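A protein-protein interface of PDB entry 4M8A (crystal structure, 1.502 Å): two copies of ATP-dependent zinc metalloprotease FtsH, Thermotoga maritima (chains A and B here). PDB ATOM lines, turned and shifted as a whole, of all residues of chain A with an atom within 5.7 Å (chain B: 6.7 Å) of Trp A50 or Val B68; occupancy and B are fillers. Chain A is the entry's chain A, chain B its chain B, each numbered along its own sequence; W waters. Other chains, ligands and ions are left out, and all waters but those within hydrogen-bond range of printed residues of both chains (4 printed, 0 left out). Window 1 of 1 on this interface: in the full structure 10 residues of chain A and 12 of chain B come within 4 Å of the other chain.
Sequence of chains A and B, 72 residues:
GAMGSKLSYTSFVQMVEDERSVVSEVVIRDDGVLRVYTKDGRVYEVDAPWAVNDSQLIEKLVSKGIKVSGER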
ATOM      1  N   SER A   8       2.734  30.889  30.428  1.00  0.00           N
ATOM      2  CA  SER A   8       2.152  30.675  29.109  1.00  0.00           C
ATOM      3  C   SER A   8       2.166  29.198  28.742  1.00  0.00           C
ATOM      4  O   SER A   8       3.004  28.423  29.237  1.00  0.00           O
ATOM      5  CB  SER A   8       2.891  31.493  28.040  1.00  0.00           C
ATOM      6  OG  SER A   8       4.174  30.923  27.831  1.00  0.00           O
ATOM      7  N   TYR A   9       1.258  28.816  27.850  1.00  0.00           N
ATOM      8  CA  TYR A   9       1.245  27.456  27.326  1.00  0.00           C
ATOM      9  C   TYR A   9       2.574  27.180  26.598  1.00  0.00           C
ATOM     10  O   TYR A   9       3.140  26.088  26.723  1.00  0.00           O
ATOM     11  CB  TYR A   9       0.022  27.216  26.421  1.00  0.00           C
ATOM     12  CG  TYR A   9      -0.046  25.794  25.935  1.00  0.00           C
ATOM     13  CD1 TYR A   9      -0.350  24.764  26.815  1.00  0.00           C
ATOM     14  CD2 TYR A   9       0.242  25.466  24.604  1.00  0.00           C
ATOM     15  CE1 TYR A   9      -0.379  23.457  26.398  1.00  0.00           C
ATOM     16  CE2 TYR A   9       0.212  24.136  24.176  1.00  0.00           C
ATOM     17  CZ  TYR A   9      -0.107  23.141  25.088  1.00  0.00           C
ATOM     18  OH  TYR A   9      -0.140  21.810  24.731  1.00  0.00           O
ATOM     19  N   THR A  10       3.079  28.163  25.847  1.00  0.00           N
ATOM     20  CA  THR A  10       4.361  27.981  25.158  1.00  0.00           C
ATOM     21  C   THR A  10       5.504  27.669  26.132  1.00  0.00           C
ATOM     22  O   THR A  10       6.288  26.738  25.924  1.00  0.00           O
ATOM     23  CB  THR A  10       4.722  29.236  24.361  1.00  0.00           C
ATOM     24  OG1 THR A  10       3.703  29.436  23.381  1.00  0.00           O
ATOM     25  CG2 THR A  10       6.105  29.075  23.683  1.00  0.00           C
ATOM     26  N   ASP A  47      -3.314  28.728  31.721  1.00  0.00           N
ATOM     27  CA  ASP A  47      -4.680  28.759  31.211  1.00  0.00           C
ATOM     28  C   ASP A  47      -4.668  28.149  29.802  1.00  0.00           C
ATOM     29  O   ASP A  47      -4.196  28.785  28.846  1.00  0.00           O
ATOM     30  CB  ASP A  47      -5.188  30.212  31.198  1.00  0.00           C
ATOM     31  CG  ASP A  47      -6.659  30.322  30.845  1.00  0.00           C
ATOM     32  OD1 ASP A  47      -7.178  29.423  30.150  1.00  0.00           O
ATOM     33  OD2 ASP A  47      -7.301  31.301  31.294  1.00  0.00           O
ATOM     34  N   ALA A  48      -5.147  26.907  29.679  1.00  0.00           N
ATOM     35  CA  ALA A  48      -5.058  26.179  28.413  1.00  0.00           C
ATOM     36  C   ALA A  48      -6.180  25.150  28.287  1.00  0.00           C
ATOM     37  O   ALA A  48      -5.949  23.946  28.422  1.00  0.00           O
ATOM     38  CB  ALA A  48      -3.685  25.483  28.284  1.00  0.00           C
ATOM     39  N   PRO A  49      -7.410  25.620  28.029  1.00  0.00           N
ATOM     40  CA  PRO A  49      -8.539  24.680  27.932  1.00  0.00           C
ATOM     41  C   PRO A  49      -8.365  23.603  26.865  1.00  0.00           C
ATOM     42  O   PRO A  49      -8.941  22.516  26.994  1.00  0.00           O
ATOM     43  CB  PRO A  49      -9.730  25.588  27.595  1.00  0.00           C
ATOM     44  CG  PRO A  49      -9.335  26.944  28.095  1.00  0.00           C
ATOM     45  CD  PRO A  49      -7.836  27.032  27.947  1.00  0.00           C
ATOM     46  N   TRP A  50      -7.557  23.889  25.850  1.00  0.00           N
ATOM     47  CA  TRP A  50      -7.289  22.939  24.775  1.00  0.00           C
ATOM     48  C   TRP A  50      -6.493  21.726  25.254  1.00  0.00           C
ATOM     49  O   TRP A  50      -6.457  20.688  24.582  1.00  0.00           O
ATOM     50  CB  TRP A  50      -6.537  23.639  23.640  1.00  0.00           C
ATOM     51  CG  TRP A  50      -5.323  24.403  24.082  1.00  0.00           C
ATOM     52  CD1 TRP A  50      -4.041  23.923  24.212  1.00  0.00           C
ATOM     53  CD2 TRP A  50      -5.269  25.794  24.447  1.00  0.00           C
ATOM     54  NE1 TRP A  50      -3.201  24.926  24.632  1.00  0.00           N
ATOM     55  CE2 TRP A  50      -3.926  26.085  24.782  1.00  0.00           C
ATOM     56  CE3 TRP A  50      -6.230  26.821  24.547  1.00  0.00           C
ATOM     57  CZ2 TRP A  50      -3.509  27.365  25.187  1.00  0.00           C
ATOM     58  CZ3 TRP A  50      -5.812  28.099  24.938  1.00  0.00           C
ATOM     59  CH2 TRP A  50      -4.464  28.354  25.269  1.00  0.00           C
ATOM     60  N   ALA A  51      -5.862  21.856  26.417  1.00  0.00           N
ATOM     61  CA  ALA A  51      -5.060  20.766  26.970  1.00  0.00           C
ATOM     62  C   ALA A  51      -5.889  19.699  27.692  1.00  0.00           C
ATOM     63  O   ALA A  51      -5.409  18.579  27.914  1.00  0.00           O
ATOM     64  CB  ALA A  51      -4.002  21.333  27.906  1.00  0.00           C
ATOM     65  N   VAL A  52      -7.121  20.031  28.057  1.00  0.00           N
ATOM     66  CA  VAL A  52      -7.980  19.063  28.730  1.00  0.00           C
ATOM     67  C   VAL A  52      -8.317  17.930  27.768  1.00  0.00           C
ATOM     68  O   VAL A  52      -8.726  18.165  26.632  1.00  0.00           O
ATOM     69  CB  VAL A  52      -9.266  19.716  29.279  1.00  0.00           C
ATOM     70  CG1 VAL A  52     -10.096  18.678  30.059  1.00  0.00           C
ATOM     71  CG2 VAL A  52      -8.906  20.914  30.153  1.00  0.00           C
ATOM     72  N   ASN A  53      -8.129  16.697  28.234  1.00  0.00           N
ATOM     73  CA  ASN A  53      -8.352  15.503  27.409  1.00  0.00           C
ATOM     74  C   ASN A  53      -7.490  15.427  26.145  1.00  0.00           C
ATOM     75  O   ASN A  53      -7.827  14.716  25.190  1.00  0.00           O
ATOM     76  CB  ASN A  53      -9.832  15.344  27.032  1.00  0.00           C
ATOM     77  CG  ASN A  53     -10.742  15.224  28.245  1.00  0.00           C
ATOM     78  OD1 ASN A  53     -11.809  15.839  28.292  1.00  0.00           O
ATOM     79  ND2 ASN A  53     -10.328  14.430  29.233  1.00  0.00           N
ATOM     80  N   ASP A  54      -6.383  16.156  26.138  1.00  0.00           N
ATOM     81  CA  ASP A  54      -5.407  16.047  25.063  1.00  0.00           C
ATOM     82  C   ASP A  54      -4.536  14.826  25.334  1.00  0.00           C
ATOM     83  O   ASP A  54      -3.584  14.891  26.126  1.00  0.00           O
ATOM     84  CB  ASP A  54      -4.559  17.324  24.986  1.00  0.00           C
ATOM     85  CG  ASP A  54      -3.546  17.301  23.843  1.00  0.00           C
ATOM     86  OD1 ASP A  54      -3.256  16.223  23.299  1.00  0.00           O
ATOM     87  OD2 ASP A  54      -3.005  18.365  23.497  1.00  0.00           O
ATOM     88  N   SER B  24       4.497  37.847  17.855  1.00  0.00           N
ATOM     89  CA  SER B  24       5.156  37.566  19.131  1.00  0.00           C
ATOM     90  C   SER B  24       4.278  36.779  20.089  1.00  0.00           C
ATOM     91  O   SER B  24       4.777  35.939  20.833  1.00  0.00           O
ATOM     92  CB  SER B  24       5.627  38.854  19.799  1.00  0.00           C
ATOM     93  OG  SER B  24       4.573  39.780  19.892  1.00  0.00           O
ATOM     94  N   GLU B  25       2.976  37.043  20.080  1.00  0.00           N
ATOM     95  CA  GLU B  25       2.095  36.438  21.071  1.00  0.00           C
ATOM     96  C   GLU B  25       0.698  36.286  20.501  1.00  0.00           C
ATOM     97  O   GLU B  25       0.219  37.154  19.764  1.00  0.00           O
ATOM     98  CB  GLU B  25       2.033  37.272  22.375  1.00  0.00           C
ATOM     99  CG  GLU B  25       1.121  36.637  23.435  1.00  0.00           C
ATOM    100  CD  GLU B  25       1.187  37.318  24.774  1.00  0.00           C
ATOM    101  OE1 GLU B  25       1.692  38.451  24.827  1.00  0.00           O
ATOM    102  OE2 GLU B  25       0.726  36.715  25.771  1.00  0.00           O
ATOM    103  N   VAL B  26       0.056  35.174  20.848  1.00  0.00           N
ATOM    104  CA  VAL B  26      -1.348  34.971  20.552  1.00  0.00           C
ATOM    105  C   VAL B  26      -2.056  34.643  21.849  1.00  0.00           C
ATOM    106  O   VAL B  26      -1.711  33.671  22.521  1.00  0.00           O
ATOM    107  CB  VAL B  26      -1.560  33.835  19.525  1.00  0.00           C
ATOM    108  CG1 VAL B  26      -3.036  33.617  19.268  1.00  0.00           C
ATOM    109  CG2 VAL B  26      -0.825  34.167  18.208  1.00  0.00           C
ATOM    110  N   VAL B  27      -3.022  35.483  22.211  1.00  0.00           N
ATOM    111  CA  VAL B  27      -3.822  35.233  23.402  1.00  0.00           C
ATOM    112  C   VAL B  27      -5.135  34.620  22.919  1.00  0.00           C
ATOM    113  O   VAL B  27      -5.865  35.225  22.124  1.00  0.00           O
ATOM    114  CB  VAL B  27      -4.089  36.525  24.229  1.00  0.00           C
ATOM    115  CG1 VAL B  27      -5.029  36.246  25.412  1.00  0.00           C
ATOM    116  CG2 VAL B  27      -2.777  37.135  24.705  1.00  0.00           C
ATOM    117  N   ILE B  28      -5.407  33.407  23.375  1.00  0.00           N
ATOM    118  CA  ILE B  28      -6.601  32.671  22.978  1.00  0.00           C
ATOM    119  C   ILE B  28      -7.653  32.884  24.069  1.00  0.00           C
ATOM    120  O   ILE B  28      -7.615  32.269  25.146  1.00  0.00           O
ATOM    121  CB  ILE B  28      -6.300  31.179  22.764  1.00  0.00           C
ATOM    122  CG1 ILE B  28      -5.174  30.999  21.731  1.00  0.00           C
ATOM    123  CG2 ILE B  28      -7.554  30.437  22.297  1.00  0.00           C
ATOM    124  CD1 ILE B  28      -4.794  29.517  21.485  1.00  0.00           C
ATOM    125  N   ARG B  29      -8.566  33.803  23.806  1.00  0.00           N
ATOM    126  CA  ARG B  29      -9.568  34.161  24.793  1.00  0.00           C
ATOM    127  C   ARG B  29     -10.685  33.136  24.823  1.00  0.00           C
ATOM    128  O   ARG B  29     -11.043  32.544  23.792  1.00  0.00           O
ATOM    129  CB  ARG B  29     -10.163  35.521  24.444  1.00  0.00           C
ATOM    130  CG  ARG B  29      -9.178  36.685  24.530  1.00  0.00           C
ATOM    131  CD  ARG B  29      -9.764  37.974  23.949  1.00  0.00           C
ATOM    132  NE  ARG B  29     -11.099  38.240  24.476  1.00  0.00           N
ATOM    133  CZ  ARG B  29     -11.341  38.948  25.569  1.00  0.00           C
ATOM    134  NH1 ARG B  29     -10.331  39.485  26.244  1.00  0.00           N
ATOM    135  NH2 ARG B  29     -12.590  39.132  25.970  1.00  0.00           N
ATOM    136  N   ALA B  51     -10.616  28.336  16.364  1.00  0.00           N
ATOM    137  CA  ALA B  51      -9.191  28.205  16.592  1.00  0.00           C
ATOM    138  C   ALA B  51      -8.861  27.700  17.990  1.00  0.00           C
ATOM    139  O   ALA B  51      -7.796  27.142  18.203  1.00  0.00           O
ATOM    140  CB  ALA B  51      -8.517  29.544  16.352  1.00  0.00           C
ATOM    141  N   VAL B  52      -9.769  27.895  18.938  1.00  0.00           N
ATOM    142  CA  VAL B  52      -9.423  27.748  20.347  1.00  0.00           C
ATOM    143  C   VAL B  52      -9.168  26.315  20.763  1.00  0.00           C
ATOM    144  O   VAL B  52      -8.584  26.070  21.820  1.00  0.00           O
ATOM    145  CB  VAL B  52     -10.501  28.353  21.259  1.00  0.00           C
ATOM    146  CG1 VAL B  52     -10.857  29.766  20.778  1.00  0.00           C
ATOM    147  CG2 VAL B  52     -11.728  27.443  21.304  1.00  0.00           C
ATOM    148  N   ASN B  53      -9.613  25.368  19.947  1.00  0.00           N
ATOM    149  CA  ASN B  53      -9.364  23.959  20.223  1.00  0.00           C
ATOM    150  C   ASN B  53      -8.677  23.260  19.063  1.00  0.00           C
ATOM    151  O   ASN B  53      -8.686  22.031  18.979  1.00  0.00           O
ATOM    152  CB  ASN B  53     -10.675  23.245  20.552  1.00  0.00           C
ATOM    153  CG  ASN B  53     -11.761  23.517  19.524  1.00  0.00           C
ATOM    154  OD1 ASN B  53     -11.478  23.785  18.354  1.00  0.00           O
ATOM    155  ND2 ASN B  53     -13.013  23.463  19.961  1.00  0.00           N
ATOM    156  N   ASP B  54      -8.093  24.049  18.165  1.00  0.00           N
ATOM    157  CA  ASP B  54      -7.365  23.514  17.018  1.00  0.00           C
ATOM    158  C   ASP B  54      -5.938  23.191  17.450  1.00  0.00           C
ATOM    159  O   ASP B  54      -5.062  24.066  17.447  1.00  0.00           O
ATOM    160  CB  ASP B  54      -7.370  24.530  15.869  1.00  0.00           C
ATOM    161  CG  ASP B  54      -6.606  24.045  14.631  1.00  0.00           C
ATOM    162  OD1 ASP B  54      -5.930  22.983  14.667  1.00  0.00           O
ATOM    163  OD2 ASP B  54      -6.678  24.745  13.602  1.00  0.00           O
ATOM    164  N   SER B  55      -5.709  21.929  17.804  1.00  0.00           N
ATOM    165  CA  SER B  55      -4.425  21.501  18.353  1.00  0.00           C
ATOM    166  C   SER B  55      -3.300  21.636  17.343  1.00  0.00           C
ATOM    167  O   SER B  55      -2.150  21.836  17.723  1.00  0.00           O
ATOM    168  CB  SER B  55      -4.499  20.052  18.838  1.00  0.00           C
ATOM    169  OG  SER B  55      -4.716  19.168  17.749  1.00  0.00           O
ATOM    170  N   LEU B  57      -3.049  24.042  15.008  1.00  0.00           N
ATOM    171  CA  LEU B  57      -2.680  25.457  15.005  1.00  0.00           C
ATOM    172  C   LEU B  57      -1.865  25.790  16.242  1.00  0.00           C
ATOM    173  O   LEU B  57      -0.835  26.457  16.170  1.00  0.00           O
ATOM    174  CB  LEU B  57      -3.919  26.346  14.968  1.00  0.00           C
ATOM    175  CG  LEU B  57      -3.667  27.844  15.212  1.00  0.00           C
ATOM    176  CD1 LEU B  57      -2.888  28.500  14.060  1.00  0.00           C
ATOM    177  CD2 LEU B  57      -4.982  28.587  15.468  1.00  0.00           C
ATOM    178  N   ILE B  58      -2.334  25.312  17.385  1.00  0.00           N
ATOM    179  CA  ILE B  58      -1.675  25.629  18.647  1.00  0.00           C
ATOM    180  C   ILE B  58      -0.256  25.080  18.713  1.00  0.00           C
ATOM    181  O   ILE B  58       0.669  25.790  19.093  1.00  0.00           O
ATOM    182  CB  ILE B  58      -2.536  25.175  19.852  1.00  0.00           C
ATOM    183  CG1 ILE B  58      -3.821  26.016  19.864  1.00  0.00           C
ATOM    184  CG2 ILE B  58      -1.774  25.341  21.157  1.00  0.00           C
ATOM    185  CD1 ILE B  58      -4.950  25.481  20.741  1.00  0.00           C
ATOM    186  N   GLU B  59      -0.056  23.830  18.335  1.00  0.00           N
ATOM    187  CA  GLU B  59       1.297  23.317  18.446  1.00  0.00           C
ATOM    188  C   GLU B  59       2.204  23.949  17.391  1.00  0.00           C
ATOM    189  O   GLU B  59       3.396  24.123  17.632  1.00  0.00           O
ATOM    190  CB  GLU B  59       1.333  21.785  18.453  1.00  0.00           C
ATOM    191  CG  GLU B  59       0.552  21.143  19.614  1.00  0.00           C
ATOM    192  CD  GLU B  59       1.060  21.517  21.013  1.00  0.00           C
ATOM    193  OE1 GLU B  59       2.281  21.735  21.196  1.00  0.00           O
ATOM    194  OE2 GLU B  59       0.230  21.558  21.947  1.00  0.00           O
ATOM    195  N   LEU B  61       1.977  27.217  16.437  1.00  0.00           N
ATOM    196  CA  LEU B  61       2.382  28.442  17.099  1.00  0.00           C
ATOM    197  C   LEU B  61       3.489  28.169  18.112  1.00  0.00           C
ATOM    198  O   LEU B  61       4.509  28.862  18.123  1.00  0.00           O
ATOM    199  CB  LEU B  61       1.185  29.066  17.813  1.00  0.00           C
ATOM    200  CG  LEU B  61       0.030  29.559  16.929  1.00  0.00           C
ATOM    201  CD1 LEU B  61      -1.124  29.995  17.811  1.00  0.00           C
ATOM    202  CD2 LEU B  61       0.468  30.679  16.000  1.00  0.00           C
ATOM    203  N   VAL B  62       3.299  27.160  18.960  1.00  0.00           N
ATOM    204  CA  VAL B  62       4.301  26.866  19.985  1.00  0.00           C
ATOM    205  C   VAL B  62       5.657  26.485  19.379  1.00  0.00           C
ATOM    206  O   VAL B  62       6.721  26.930  19.844  1.00  0.00           O
ATOM    207  CB  VAL B  62       3.807  25.763  20.966  1.00  0.00           C
ATOM    208  CG1 VAL B  62       4.932  25.320  21.911  1.00  0.00           C
ATOM    209  CG2 VAL B  62       2.608  26.261  21.752  1.00  0.00           C
ATOM    210  N   GLY B  65       7.828  29.200  18.502  1.00  0.00           N
ATOM    211  CA  GLY B  65       8.275  29.994  19.629  1.00  0.00           C
ATOM    212  C   GLY B  65       7.365  31.167  19.917  1.00  0.00           C
ATOM    213  O   GLY B  65       7.697  32.010  20.749  1.00  0.00           O
ATOM    214  N   ILE B  66       6.208  31.212  19.246  1.00  0.00           N
ATOM    215  CA  ILE B  66       5.207  32.250  19.506  1.00  0.00           C
ATOM    216  C   ILE B  66       4.611  31.982  20.878  1.00  0.00           C
ATOM    217  O   ILE B  66       4.344  30.835  21.231  1.00  0.00           O
ATOM    218  CB  ILE B  66       4.120  32.273  18.411  1.00  0.00           C
ATOM    219  CG1 ILE B  66       4.750  32.690  17.072  1.00  0.00           C
ATOM    220  CG2 ILE B  66       2.949  33.195  18.809  1.00  0.00           C
ATOM    221  CD1 ILE B  66       3.884  32.422  15.870  1.00  0.00           C
ATOM    222  N   LYS B  67       4.470  33.028  21.679  1.00  0.00           N
ATOM    223  CA  LYS B  67       3.899  32.885  23.008  1.00  0.00           C
ATOM    224  C   LYS B  67       2.403  32.668  22.884  1.00  0.00           C
ATOM    225  O   LYS B  67       1.691  33.515  22.340  1.00  0.00           O
ATOM    226  CB  LYS B  67       4.182  34.137  23.839  1.00  0.00           C
ATOM    227  CG  LYS B  67       3.682  34.052  25.275  1.00  0.00           C
ATOM    228  CD  LYS B  67       4.141  35.282  26.070  1.00  0.00           C
ATOM    229  CE  LYS B  67       3.660  35.201  27.514  1.00  0.00           C
ATOM    230  NZ  LYS B  67       4.010  36.451  28.264  1.00  0.00           N
ATOM    231  N   VAL B  68       1.916  31.543  23.393  1.00  0.00           N
ATOM    232  CA  VAL B  68       0.488  31.237  23.360  1.00  0.00           C
ATOM    233  C   VAL B  68      -0.030  31.236  24.789  1.00  0.00           C
ATOM    234  O   VAL B  68       0.512  30.529  25.648  1.00  0.00           O
ATOM    235  CB  VAL B  68       0.226  29.860  22.725  1.00  0.00           C
ATOM    236  CG1 VAL B  68      -1.259  29.513  22.799  1.00  0.00           C
ATOM    237  CG2 VAL B  68       0.746  29.841  21.290  1.00  0.00           C
ATOM    238  N   SER B  69      -1.074  32.021  25.038  1.00  0.00           N
ATOM    239  CA  SER B  69      -1.610  32.258  26.386  1.00  0.00           C
ATOM    240  C   SER B  69      -3.119  32.166  26.329  1.00  0.00           C
ATOM    241  O   SER B  69      -3.731  32.837  25.504  1.00  0.00           O
ATOM    242  CB  SER B  69      -1.277  33.688  26.846  1.00  0.00           C
ATOM    243  OG  SER B  69       0.134  33.937  26.796  1.00  0.00           O
ATOM    244  N   GLY B  70      -3.725  31.372  27.205  1.00  0.00           N
ATOM    245  CA  GLY B  70      -5.167  31.406  27.364  1.00  0.00           C
ATOM    246  C   GLY B  70      -5.624  32.588  28.202  1.00  0.00           C
ATOM    247  O   GLY B  70      -4.856  33.123  29.003  1.00  0.00           O
ATOM    248  N   GLU B  71      -6.874  32.998  28.026  1.00  0.00           N
ATOM    249  CA  GLU B  71      -7.425  34.114  28.791  1.00  0.00           C
ATOM    250  C   GLU B  71      -8.864  33.794  29.149  1.00  0.00           C
ATOM    251  O   GLU B  71      -9.554  33.120  28.386  1.00  0.00           O
ATOM    252  CB  GLU B  71      -7.359  35.424  27.976  1.00  0.00           C
ATOM    253  CG  GLU B  71      -7.902  36.688  28.679  1.00  0.00           C
ATOM    254  CD  GLU B  71      -9.425  36.864  28.578  1.00  0.00           C
ATOM    255  OE1 GLU B  71     -10.078  36.181  27.756  1.00  0.00           O
ATOM    256  OE2 GLU B  71      -9.982  37.688  29.337  1.00  0.00           O
HETATM  257  O   HOH W   1      -1.706  29.668  28.495  1.00  0.00           O
HETATM  258  O   HOH W   2      -9.338  30.306  28.737  1.00  0.00           O
HETATM  259  O   HOH W   3      -9.889  25.844  24.139  1.00  0.00           O
HETATM  260  O   HOH W   4      -0.759  18.426  22.353  1.00  0.00           O
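OH of Tyr A9 sits at hydrogen-bond distance from OE2 of Glu B59. The backbone carbonyl oxygen of Val B68 is in hydrogen-bond range of the backbone NH of Tyr A9, at 2.9 Å. The side-chain hydroxyl (OG1) of Thr A10 sits at hydrogen-bond distance from the backbone carbonyl oxygen (O) of Ile B66, at 2.6 Å. The backbone NH of Val B68 lies within hydrogen-bond range of the side-chain hydroxyl of Thr A10, 2.8 Å away. O of Asp A47 lies within hydrogen-bond range of N of Gly B70, at 3.1 Å.
N of Lys B67 lies within hydrogen-bond range of O of Ser B24 (3.0 Å). The side-chain carboxylate (OE2) of Glu B25 is in hydrogen-bond range of the side-chain hydroxyl (OG) of Ser B69. The backbone NH of Val B26 sits at hydrogen-bond distance from the backbone carbonyl oxygen of Lys B67, 2.8 Å away. O of Val B26 lies within hydrogen-bond range of N of Ser B69, at 3.1 Å. The backbone carbonyl oxygen (O) of Ser B69 lies within hydrogen-bond range of the backbone NH (N) of Ile B28. The backbone NH (N) of Ile B66 is in hydrogen-bond range of the backbone carbonyl oxygen (O) of Leu B61 (3.1 Å).
Among the printed residues, pairs that only touch across the chains: Thr A10 with Lys B67, Ser A8 with Val B68, Trp A50 with Ile B58, Asp A47 with Glu B71, Trp A50 with Gly B70, Trp A50 with Val B52, Thr A10 with Val B62, Tyr A9 with Val B62, Trp A50 with Ile B28, Tyr A9 with Ile B58, Ser A8 with Lys B67, Ser A8 with Ser B69 and Trp A50 with Val B68.
Of chain B, only Ile B28, Val B52, Ile B58, Val B68 and Gly B70 come within 4 Å of Trp A50. Of chain A, only Ser A8 (3.5 Å), Tyr A9 (2.9 Å), Thr A10 (2.8 Å) and Trp A50 (3.9 Å) come within 4 Å of Val B68. Of the printed residues of chain A, Val B62 touches Tyr A9 and Thr A10. Printed residues of chain A within 4 Å of Ile B28: Trp A50 (3.8 Å). Printed residues of chain A within 4 Å of Ser B69: Ser A8. The nearest printed residue of chain A that does not touch Gly B70 is Ala A48 (5.1 Å).
Of the 23 printed residues of chain B, 11 touch a printed residue of chain A. Hydrophobic or aromatic side chains of chain B that line the printed part of chain A: Ile B28, Ile B58, Val B62 and Val B68. Of the 11 printed residues of chain A, 5 touch a printed residue of chain B. Among the printed residues, 18 pairs touch across the chains.
Positions printed for both chains: 51, 52, 53 and 54.
Water W4 bridges OD2 of Asp A54 and OE2 of Glu B59. Water W1 lies within hydrogen-bond range of O of Asp A47, N of Gly B70 and N of Tyr A9. Water W3 bridges O of Val B52 (2.7 Å) and N of Trp A50 (3.5 Å). Water W2 lies within hydrogen-bond range of the side-chain carboxylate of Asp A47 and the backbone carbonyl oxygen of Glu B71.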
